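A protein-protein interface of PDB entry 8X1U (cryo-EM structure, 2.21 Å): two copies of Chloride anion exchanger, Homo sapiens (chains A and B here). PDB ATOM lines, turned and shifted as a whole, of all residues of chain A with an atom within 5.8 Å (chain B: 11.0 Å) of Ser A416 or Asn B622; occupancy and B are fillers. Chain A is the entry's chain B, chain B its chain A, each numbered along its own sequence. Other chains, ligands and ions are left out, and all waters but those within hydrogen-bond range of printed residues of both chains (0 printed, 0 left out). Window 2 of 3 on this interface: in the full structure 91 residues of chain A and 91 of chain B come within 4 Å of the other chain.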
ATOM      1  N   LYS A 294      -8.430  30.433   8.822  1.00  0.00           N
ATOM      2  CA  LYS A 294      -7.447  29.367   8.889  1.00  0.00           C
ATOM      3  C   LYS A 294      -6.095  29.879   8.462  1.00  0.00           C
ATOM      4  O   LYS A 294      -5.087  29.596   9.103  1.00  0.00           O
ATOM      5  CB  LYS A 294      -7.861  28.198   7.996  1.00  0.00           C
ATOM      6  CG  LYS A 294      -7.014  26.955   8.198  1.00  0.00           C
ATOM      7  CD  LYS A 294      -7.671  25.725   7.597  1.00  0.00           C
ATOM      8  CE  LYS A 294      -6.941  24.460   8.021  1.00  0.00           C
ATOM      9  NZ  LYS A 294      -7.603  23.226   7.515  1.00  0.00           N
ATOM     10  N   ASP A 295      -6.056  30.633   7.374  1.00  0.00           N
ATOM     11  CA  ASP A 295      -4.784  31.154   6.899  1.00  0.00           C
ATOM     12  C   ASP A 295      -4.147  32.078   7.927  1.00  0.00           C
ATOM     13  O   ASP A 295      -2.945  32.012   8.163  1.00  0.00           O
ATOM     14  CB  ASP A 295      -4.936  31.795   5.528  1.00  0.00           C
ATOM     15  CG  ASP A 295      -4.996  30.762   4.423  1.00  0.00           C
ATOM     16  OD1 ASP A 295      -4.178  29.817   4.459  1.00  0.00           O
ATOM     17  OD2 ASP A 295      -5.859  30.884   3.529  1.00  0.00           O
ATOM     18  N   PRO A 298      -2.283  30.609  13.138  1.00  0.00           N
ATOM     19  CA  PRO A 298      -1.051  29.822  13.125  1.00  0.00           C
ATOM     20  C   PRO A 298      -1.389  28.383  13.415  1.00  0.00           C
ATOM     21  O   PRO A 298      -0.880  27.482  12.752  1.00  0.00           O
ATOM     22  CB  PRO A 298      -0.249  30.414  14.280  1.00  0.00           C
ATOM     23  CG  PRO A 298      -1.262  31.041  15.177  1.00  0.00           C
ATOM     24  CD  PRO A 298      -2.338  31.551  14.267  1.00  0.00           C
ATOM     25  N   PRO A 300      -4.900  25.854  14.557  1.00  0.00           N
ATOM     26  CA  PRO A 300      -6.329  25.878  14.866  1.00  0.00           C
ATOM     27  C   PRO A 300      -6.568  26.095  16.351  1.00  0.00           C
ATOM     28  O   PRO A 300      -5.825  25.545  17.160  1.00  0.00           O
ATOM     29  CB  PRO A 300      -6.801  24.477  14.460  1.00  0.00           C
ATOM     30  CG  PRO A 300      -5.574  23.695  14.111  1.00  0.00           C
ATOM     31  CD  PRO A 300      -4.526  24.692  13.740  1.00  0.00           C
ATOM     32  N   LYS A 375      -3.878  14.201  -1.708  1.00  0.00           N
ATOM     33  CA  LYS A 375      -3.382  15.535  -1.395  1.00  0.00           C
ATOM     34  C   LYS A 375      -1.858  15.614  -1.258  1.00  0.00           C
ATOM     35  O   LYS A 375      -1.259  16.604  -1.642  1.00  0.00           O
ATOM     36  CB  LYS A 375      -4.029  16.077  -0.130  1.00  0.00           C
ATOM     37  CG  LYS A 375      -3.438  17.392   0.326  1.00  0.00           C
ATOM     38  CD  LYS A 375      -4.197  17.944   1.511  1.00  0.00           C
ATOM     39  CE  LYS A 375      -3.688  19.314   1.904  1.00  0.00           C
ATOM     40  NZ  LYS A 375      -4.510  19.907   2.988  1.00  0.00           N
ATOM     41  N   TYR A 376      -1.234  14.595  -0.679  1.00  0.00           N
ATOM     42  CA  TYR A 376       0.217  14.599  -0.487  1.00  0.00           C
ATOM     43  C   TYR A 376       1.022  13.714  -1.429  1.00  0.00           C
ATOM     44  O   TYR A 376       2.203  13.492  -1.203  1.00  0.00           O
ATOM     45  CB  TYR A 376       0.583  14.323   0.967  1.00  0.00           C
ATOM     46  CG  TYR A 376       0.039  15.370   1.897  1.00  0.00           C
ATOM     47  CD1 TYR A 376      -1.156  15.176   2.562  1.00  0.00           C
ATOM     48  CD2 TYR A 376       0.704  16.564   2.084  1.00  0.00           C
ATOM     49  CE1 TYR A 376      -1.663  16.138   3.401  1.00  0.00           C
ATOM     50  CE2 TYR A 376       0.204  17.530   2.922  1.00  0.00           C
ATOM     51  CZ  TYR A 376      -0.979  17.306   3.577  1.00  0.00           C
ATOM     52  OH  TYR A 376      -1.484  18.261   4.412  1.00  0.00           O
ATOM     53  N   SER A 411      -8.849  13.159  12.341  1.00  0.00           N
ATOM     54  CA  SER A 411      -7.831  13.157  11.287  1.00  0.00           C
ATOM     55  C   SER A 411      -7.668  14.564  10.734  1.00  0.00           C
ATOM     56  O   SER A 411      -6.549  15.047  10.643  1.00  0.00           O
ATOM     57  CB  SER A 411      -8.147  12.133  10.192  1.00  0.00           C
ATOM     58  OG  SER A 411      -8.222  10.828  10.729  1.00  0.00           O
ATOM     59  N   ALA A 412      -8.759  15.221  10.338  1.00  0.00           N
ATOM     60  CA  ALA A 412      -8.633  16.620   9.951  1.00  0.00           C
ATOM     61  C   ALA A 412      -7.880  17.417  11.006  1.00  0.00           C
ATOM     62  O   ALA A 412      -7.099  18.310  10.670  1.00  0.00           O
ATOM     63  CB  ALA A 412     -10.014  17.221   9.710  1.00  0.00           C
ATOM     64  N   VAL A 413      -8.110  17.123  12.286  1.00  0.00           N
ATOM     65  CA  VAL A 413      -7.361  17.802  13.343  1.00  0.00           C
ATOM     66  C   VAL A 413      -5.884  17.432  13.276  1.00  0.00           C
ATOM     67  O   VAL A 413      -5.007  18.241  13.601  1.00  0.00           O
ATOM     68  CB  VAL A 413      -7.962  17.488  14.724  1.00  0.00           C
ATOM     69  CG1 VAL A 413      -7.220  18.239  15.804  1.00  0.00           C
ATOM     70  CG2 VAL A 413      -9.415  17.889  14.763  1.00  0.00           C
ATOM     71  N   GLN A 414      -5.582  16.202  12.855  1.00  0.00           N
ATOM     72  CA  GLN A 414      -4.186  15.785  12.775  1.00  0.00           C
ATOM     73  C   GLN A 414      -3.493  16.391  11.567  1.00  0.00           C
ATOM     74  O   GLN A 414      -2.335  16.809  11.653  1.00  0.00           O
ATOM     75  CB  GLN A 414      -4.078  14.263  12.729  1.00  0.00           C
ATOM     76  CG  GLN A 414      -2.669  13.771  12.983  1.00  0.00           C
ATOM     77  CD  GLN A 414      -2.495  12.295  12.730  1.00  0.00           C
ATOM     78  OE1 GLN A 414      -3.468  11.505  13.159  1.00  0.00           O
ATOM     79  NE2 GLN A 414      -1.503  11.868  12.152  1.00  0.00           N
ATOM     80  N   GLU A 415      -4.179  16.442  10.426  1.00  0.00           N
ATOM     81  CA  GLU A 415      -3.566  16.961   9.210  1.00  0.00           C
ATOM     82  C   GLU A 415      -3.481  18.481   9.229  1.00  0.00           C
ATOM     83  O   GLU A 415      -2.485  19.054   8.774  1.00  0.00           O
ATOM     84  CB  GLU A 415      -4.353  16.487   7.990  1.00  0.00           C
ATOM     85  CG  GLU A 415      -3.814  16.992   6.664  1.00  0.00           C
ATOM     86  CD  GLU A 415      -4.615  18.153   6.104  1.00  0.00           C
ATOM     87  OE1 GLU A 415      -5.819  18.262   6.414  1.00  0.00           O
ATOM     88  OE2 GLU A 415      -4.037  18.959   5.347  1.00  0.00           O
ATOM     89  N   SER A 416      -4.508  19.147   9.748  1.00  0.00           N
ATOM     90  CA  SER A 416      -4.563  20.599   9.793  1.00  0.00           C
ATOM     91  C   SER A 416      -3.553  21.209  10.750  1.00  0.00           C
ATOM     92  O   SER A 416      -3.231  22.392  10.609  1.00  0.00           O
ATOM     93  CB  SER A 416      -5.969  21.047  10.190  1.00  0.00           C
ATOM     94  OG  SER A 416      -5.944  22.344  10.754  1.00  0.00           O
ATOM     95  N   THR A 417      -3.124  20.428  11.730  1.00  0.00           N
ATOM     96  CA  THR A 417      -2.202  20.880  12.755  1.00  0.00           C
ATOM     97  C   THR A 417      -0.754  20.488  12.490  1.00  0.00           C
ATOM     98  O   THR A 417       0.057  20.462  13.390  1.00  0.00           O
ATOM     99  CB  THR A 417      -2.660  20.382  14.142  1.00  0.00           C
ATOM    100  OG1 THR A 417      -2.725  18.960  14.154  1.00  0.00           O
ATOM    101  CG2 THR A 417      -4.007  20.931  14.503  1.00  0.00           C
ATOM    102  N   GLY A 418      -0.438  20.173  11.246  1.00  0.00           N
ATOM    103  CA  GLY A 418       0.919  19.844  10.872  1.00  0.00           C
ATOM    104  C   GLY A 418       1.346  18.403  10.840  1.00  0.00           C
ATOM    105  O   GLY A 418       2.524  18.131  10.904  1.00  0.00           O
ATOM    106  N   GLY A 419       0.405  17.479  10.729  1.00  0.00           N
ATOM    107  CA  GLY A 419       0.741  16.072  10.694  1.00  0.00           C
ATOM    108  C   GLY A 419       1.466  15.684   9.427  1.00  0.00           C
ATOM    109  O   GLY A 419       0.913  15.790   8.331  1.00  0.00           O
ATOM    110  N   ARG B 587       7.009  28.739  -8.847  1.00  0.00           N
ATOM    111  CA  ARG B 587       7.235  29.418  -7.577  1.00  0.00           C
ATOM    112  C   ARG B 587       8.708  29.748  -7.390  1.00  0.00           C
ATOM    113  O   ARG B 587       9.057  30.867  -6.996  1.00  0.00           O
ATOM    114  CB  ARG B 587       6.733  28.555  -6.423  1.00  0.00           C
ATOM    115  CG  ARG B 587       5.229  28.497  -6.298  1.00  0.00           C
ATOM    116  CD  ARG B 587       4.815  27.674  -5.095  1.00  0.00           C
ATOM    117  NE  ARG B 587       3.705  28.285  -4.377  1.00  0.00           N
ATOM    118  CZ  ARG B 587       3.846  29.152  -3.382  1.00  0.00           C
ATOM    119  NH1 ARG B 587       5.055  29.515  -2.984  1.00  0.00           N
ATOM    120  NH2 ARG B 587       2.776  29.659  -2.789  1.00  0.00           N
ATOM    121  N   GLU B 618       9.214  23.831   0.910  1.00  0.00           N
ATOM    122  CA  GLU B 618       8.572  23.065   1.995  1.00  0.00           C
ATOM    123  C   GLU B 618       7.251  23.661   2.377  1.00  0.00           C
ATOM    124  O   GLU B 618       7.100  24.248   3.439  1.00  0.00           O
ATOM    125  CB  GLU B 618       9.449  22.913   3.246  1.00  0.00           C
ATOM    126  CG  GLU B 618      10.679  22.068   3.065  1.00  0.00           C
ATOM    127  CD  GLU B 618      11.592  21.971   4.281  1.00  0.00           C
ATOM    128  OE1 GLU B 618      11.407  22.707   5.270  1.00  0.00           O
ATOM    129  OE2 GLU B 618      12.569  21.195   4.206  1.00  0.00           O
ATOM    130  N   LEU B 619       6.288  23.540   1.488  1.00  0.00           N
ATOM    131  CA  LEU B 619       4.970  24.072   1.799  1.00  0.00           C
ATOM    132  C   LEU B 619       4.297  23.229   2.874  1.00  0.00           C
ATOM    133  O   LEU B 619       4.504  22.017   2.964  1.00  0.00           O
ATOM    134  CB  LEU B 619       4.102  24.109   0.543  1.00  0.00           C
ATOM    135  CG  LEU B 619       4.357  25.245  -0.448  1.00  0.00           C
ATOM    136  CD1 LEU B 619       5.504  24.905  -1.379  1.00  0.00           C
ATOM    137  CD2 LEU B 619       3.103  25.539  -1.239  1.00  0.00           C
ATOM    138  N   ASP B 620       3.485  23.881   3.697  1.00  0.00           N
ATOM    139  CA  ASP B 620       2.836  23.193   4.799  1.00  0.00           C
ATOM    140  C   ASP B 620       1.490  22.619   4.366  1.00  0.00           C
ATOM    141  O   ASP B 620       1.079  22.732   3.210  1.00  0.00           O
ATOM    142  CB  ASP B 620       2.654  24.128   5.992  1.00  0.00           C
ATOM    143  CG  ASP B 620       1.786  25.318   5.672  1.00  0.00           C
ATOM    144  OD1 ASP B 620       2.102  26.033   4.701  1.00  0.00           O
ATOM    145  OD2 ASP B 620       0.791  25.541   6.392  1.00  0.00           O
ATOM    146  N   ASN B 621       0.808  21.991   5.322  1.00  0.00           N
ATOM    147  CA  ASN B 621      -0.396  21.234   5.013  1.00  0.00           C
ATOM    148  C   ASN B 621      -1.551  22.117   4.570  1.00  0.00           C
ATOM    149  O   ASN B 621      -2.455  21.636   3.880  1.00  0.00           O
ATOM    150  CB  ASN B 621      -0.816  20.412   6.233  1.00  0.00           C
ATOM    151  CG  ASN B 621       0.183  19.332   6.577  1.00  0.00           C
ATOM    152  OD1 ASN B 621       1.390  19.521   6.446  1.00  0.00           O
ATOM    153  ND2 ASN B 621      -0.316  18.187   7.019  1.00  0.00           N
ATOM    154  N   ASN B 622      -1.547  23.392   4.947  1.00  0.00           N
ATOM    155  CA  ASN B 622      -2.635  24.301   4.615  1.00  0.00           C
ATOM    156  C   ASN B 622      -2.305  25.216   3.448  1.00  0.00           C
ATOM    157  O   ASN B 622      -3.151  26.024   3.054  1.00  0.00           O
ATOM    158  CB  ASN B 622      -3.015  25.136   5.839  1.00  0.00           C
ATOM    159  CG  ASN B 622      -3.393  24.281   7.030  1.00  0.00           C
ATOM    160  OD1 ASN B 622      -4.130  23.304   6.899  1.00  0.00           O
ATOM    161  ND2 ASN B 622      -2.891  24.645   8.204  1.00  0.00           N
ATOM    162  N   GLN B 623      -1.096  25.119   2.917  1.00  0.00           N
ATOM    163  CA  GLN B 623      -0.717  25.930   1.776  1.00  0.00           C
ATOM    164  C   GLN B 623      -0.330  25.070   0.590  1.00  0.00           C
ATOM    165  O   GLN B 623      -0.157  25.579  -0.510  1.00  0.00           O
ATOM    166  CB  GLN B 623       0.442  26.838   2.157  1.00  0.00           C
ATOM    167  CG  GLN B 623       0.084  27.879   3.201  1.00  0.00           C
ATOM    168  CD  GLN B 623       1.291  28.656   3.681  1.00  0.00           C
ATOM    169  OE1 GLN B 623       2.419  28.388   3.271  1.00  0.00           O
ATOM    170  NE2 GLN B 623       1.058  29.629   4.553  1.00  0.00           N
ATOM    171  N   ILE B 624      -0.202  23.769   0.800  1.00  0.00           N
ATOM    172  CA  ILE B 624       0.236  22.879  -0.268  1.00  0.00           C
ATOM    173  C   ILE B 624      -0.751  22.817  -1.430  1.00  0.00           C
ATOM    174  O   ILE B 624      -0.362  22.511  -2.551  1.00  0.00           O
ATOM    175  CB  ILE B 624       0.493  21.458   0.278  1.00  0.00           C
ATOM    176  CG1 ILE B 624       1.238  20.612  -0.755  1.00  0.00           C
ATOM    177  CG2 ILE B 624      -0.813  20.796   0.695  1.00  0.00           C
ATOM    178  CD1 ILE B 624       1.553  19.211  -0.283  1.00  0.00           C
ATOM    179  N   GLU B 625      -2.018  23.114  -1.175  1.00  0.00           N
ATOM    180  CA  GLU B 625      -3.038  23.017  -2.218  1.00  0.00           C
ATOM    181  C   GLU B 625      -2.789  23.988  -3.359  1.00  0.00           C
ATOM    182  O   GLU B 625      -3.300  23.798  -4.458  1.00  0.00           O
ATOM    183  CB  GLU B 625      -4.424  23.249  -1.622  1.00  0.00           C
ATOM    184  CG  GLU B 625      -4.547  24.552  -0.852  1.00  0.00           C
ATOM    185  CD  GLU B 625      -5.848  24.650  -0.081  1.00  0.00           C
ATOM    186  OE1 GLU B 625      -6.646  23.691  -0.135  1.00  0.00           O
ATOM    187  OE2 GLU B 625      -6.071  25.684   0.583  1.00  0.00           O
ATOM    188  N   VAL B 626      -2.008  25.027  -3.105  1.00  0.00           N
ATOM    189  CA  VAL B 626      -1.692  26.004  -4.136  1.00  0.00           C
ATOM    190  C   VAL B 626      -0.997  25.383  -5.356  1.00  0.00           C
ATOM    191  O   VAL B 626      -0.898  26.018  -6.399  1.00  0.00           O
ATOM    192  CB  VAL B 626      -0.806  27.129  -3.562  1.00  0.00           C
ATOM    193  CG1 VAL B 626       0.624  26.645  -3.392  1.00  0.00           C
ATOM    194  CG2 VAL B 626      -0.851  28.355  -4.457  1.00  0.00           C
ATOM    195  N   LEU B 627      -0.527  24.146  -5.240  1.00  0.00           N
ATOM    196  CA  LEU B 627       0.194  23.538  -6.348  1.00  0.00           C
ATOM    197  C   LEU B 627      -0.728  22.921  -7.390  1.00  0.00           C
ATOM    198  O   LEU B 627      -0.248  22.531  -8.458  1.00  0.00           O
ATOM    199  CB  LEU B 627       1.159  22.470  -5.830  1.00  0.00           C
ATOM    200  CG  LEU B 627       2.255  22.934  -4.875  1.00  0.00           C
ATOM    201  CD1 LEU B 627       3.261  21.827  -4.657  1.00  0.00           C
ATOM    202  CD2 LEU B 627       2.938  24.176  -5.400  1.00  0.00           C
ATOM    203  N   ASP B 628      -2.024  22.823  -7.120  1.00  0.00           N
ATOM    204  CA  ASP B 628      -2.971  22.250  -8.064  1.00  0.00           C
ATOM    205  C   ASP B 628      -3.728  23.307  -8.856  1.00  0.00           C
ATOM    206  O   ASP B 628      -4.674  22.967  -9.572  1.00  0.00           O
ATOM    207  CB  ASP B 628      -3.965  21.348  -7.333  1.00  0.00           C
ATOM    208  CG  ASP B 628      -3.287  20.352  -6.422  1.00  0.00           C
ATOM    209  OD1 ASP B 628      -2.041  20.357  -6.359  1.00  0.00           O
ATOM    210  OD2 ASP B 628      -3.995  19.564  -5.764  1.00  0.00           O
ATOM    211  N   GLN B 629      -3.339  24.563  -8.746  1.00  0.00           N
ATOM    212  CA  GLN B 629      -4.009  25.658  -9.429  1.00  0.00           C
ATOM    213  C   GLN B 629      -3.487  25.805 -10.853  1.00  0.00           C
ATOM    214  O   GLN B 629      -2.339  25.455 -11.139  1.00  0.00           O
ATOM    215  CB  GLN B 629      -3.797  26.963  -8.672  1.00  0.00           C
ATOM    216  CG  GLN B 629      -4.321  26.943  -7.249  1.00  0.00           C
ATOM    217  CD  GLN B 629      -5.743  26.433  -7.155  1.00  0.00           C
ATOM    218  OE1 GLN B 629      -6.609  26.824  -7.938  1.00  0.00           O
ATOM    219  NE2 GLN B 629      -5.992  25.551  -6.194  1.00  0.00           N
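The backbone carbonyl oxygen (O) of Gly A419 lies within hydrogen-bond range of the side-chain amide nitrogen (ND2) of Asn B621 (3.0 Å).
ND2 of Asn B622 sits at hydrogen-bond distance from O of Ser A416 (3.3 Å).
ND2 of Asn B621 is in hydrogen-bond range of OH of Tyr A376 (2.9 Å).
NZ of Lys A375 sits at hydrogen-bond distance from O of Asn B621 (2.8 Å).
The side-chain amide nitrogen (ND2) of Asn B621 sits at hydrogen-bond distance from the backbone carbonyl oxygen (O) of Glu A415 (2.9 Å).
OD2 of Asp B620 lies close to N of Asn B622 (3.5 Å).
OE2 of Glu A415 lies within salt-bridge range of NZ of Lys A375, at 2.6 Å.
The backbone carbonyl oxygen (O) of Gln A414 sits at hydrogen-bond distance from the backbone NH (N) of Gly A419.
The side-chain hydroxyl (OH) of Tyr A376 is in hydrogen-bond range of the side-chain carboxylate (OE2) of Glu A415.
Among the printed residues, merely in contact across the chains: Lys A294 with Asn B622, Lys A375 with Ile B624 and Tyr A376 with Ile B624.
Of chain A, only Lys A294 (3.2 Å) and Ser A416 (3.3 Å) come within 4 Å of Asn B622.
No residue of chain B comes within 4 Å of Ala A412.
No residue of chain B comes within 4 Å of Val A413.
No residue of chain B comes within 4 Å of Gly A418.
Gly A419 touches just one residue of chain B: Asn B621.
Printed residues of chain A within 4 Å of Ile B624: Lys A375 and Tyr A376.
Of the printed residues of chain B, Tyr A376 touches Asn B621 and Ile B624.
Printed residues of chain A within 4 Å of Asn B621: Lys A375, Tyr A376, Glu A415 and Gly A419.
Printed residues of chain B within 4 Å of Lys A375: Asn B621 (2.8 Å) and Ile B624 (3.5 Å).
Asp A295 touches none of the printed residues of chain B.
Pro A300 touches none of the printed residues of chain B.
The nearest residue of chain B that does not touch Ser A416 is Asn B621 (5.1 Å).
The nearest printed residue of chain B that does not touch Lys A375 is Asn B622 (5.0 Å).
Printed residues of chain B that touch a printed residue of chain A: Asn B621, Asn B622 and Ile B624.
Of the 15 printed residues of chain A, 6 touch a printed residue of chain B.
Hydrophobic or aromatic side chains of chain A within 4 Å of the printed part of chain B: Tyr A376.
Among the printed residues, no Asp or Glu carboxylate lies within 4 Å of a Lys or Arg side-chain nitrogen of the other chain.
No position is printed for both chains.
Of the 8 pairs that touch across the chains among the printed residues, none has its exchanged pair printed and touching as well.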
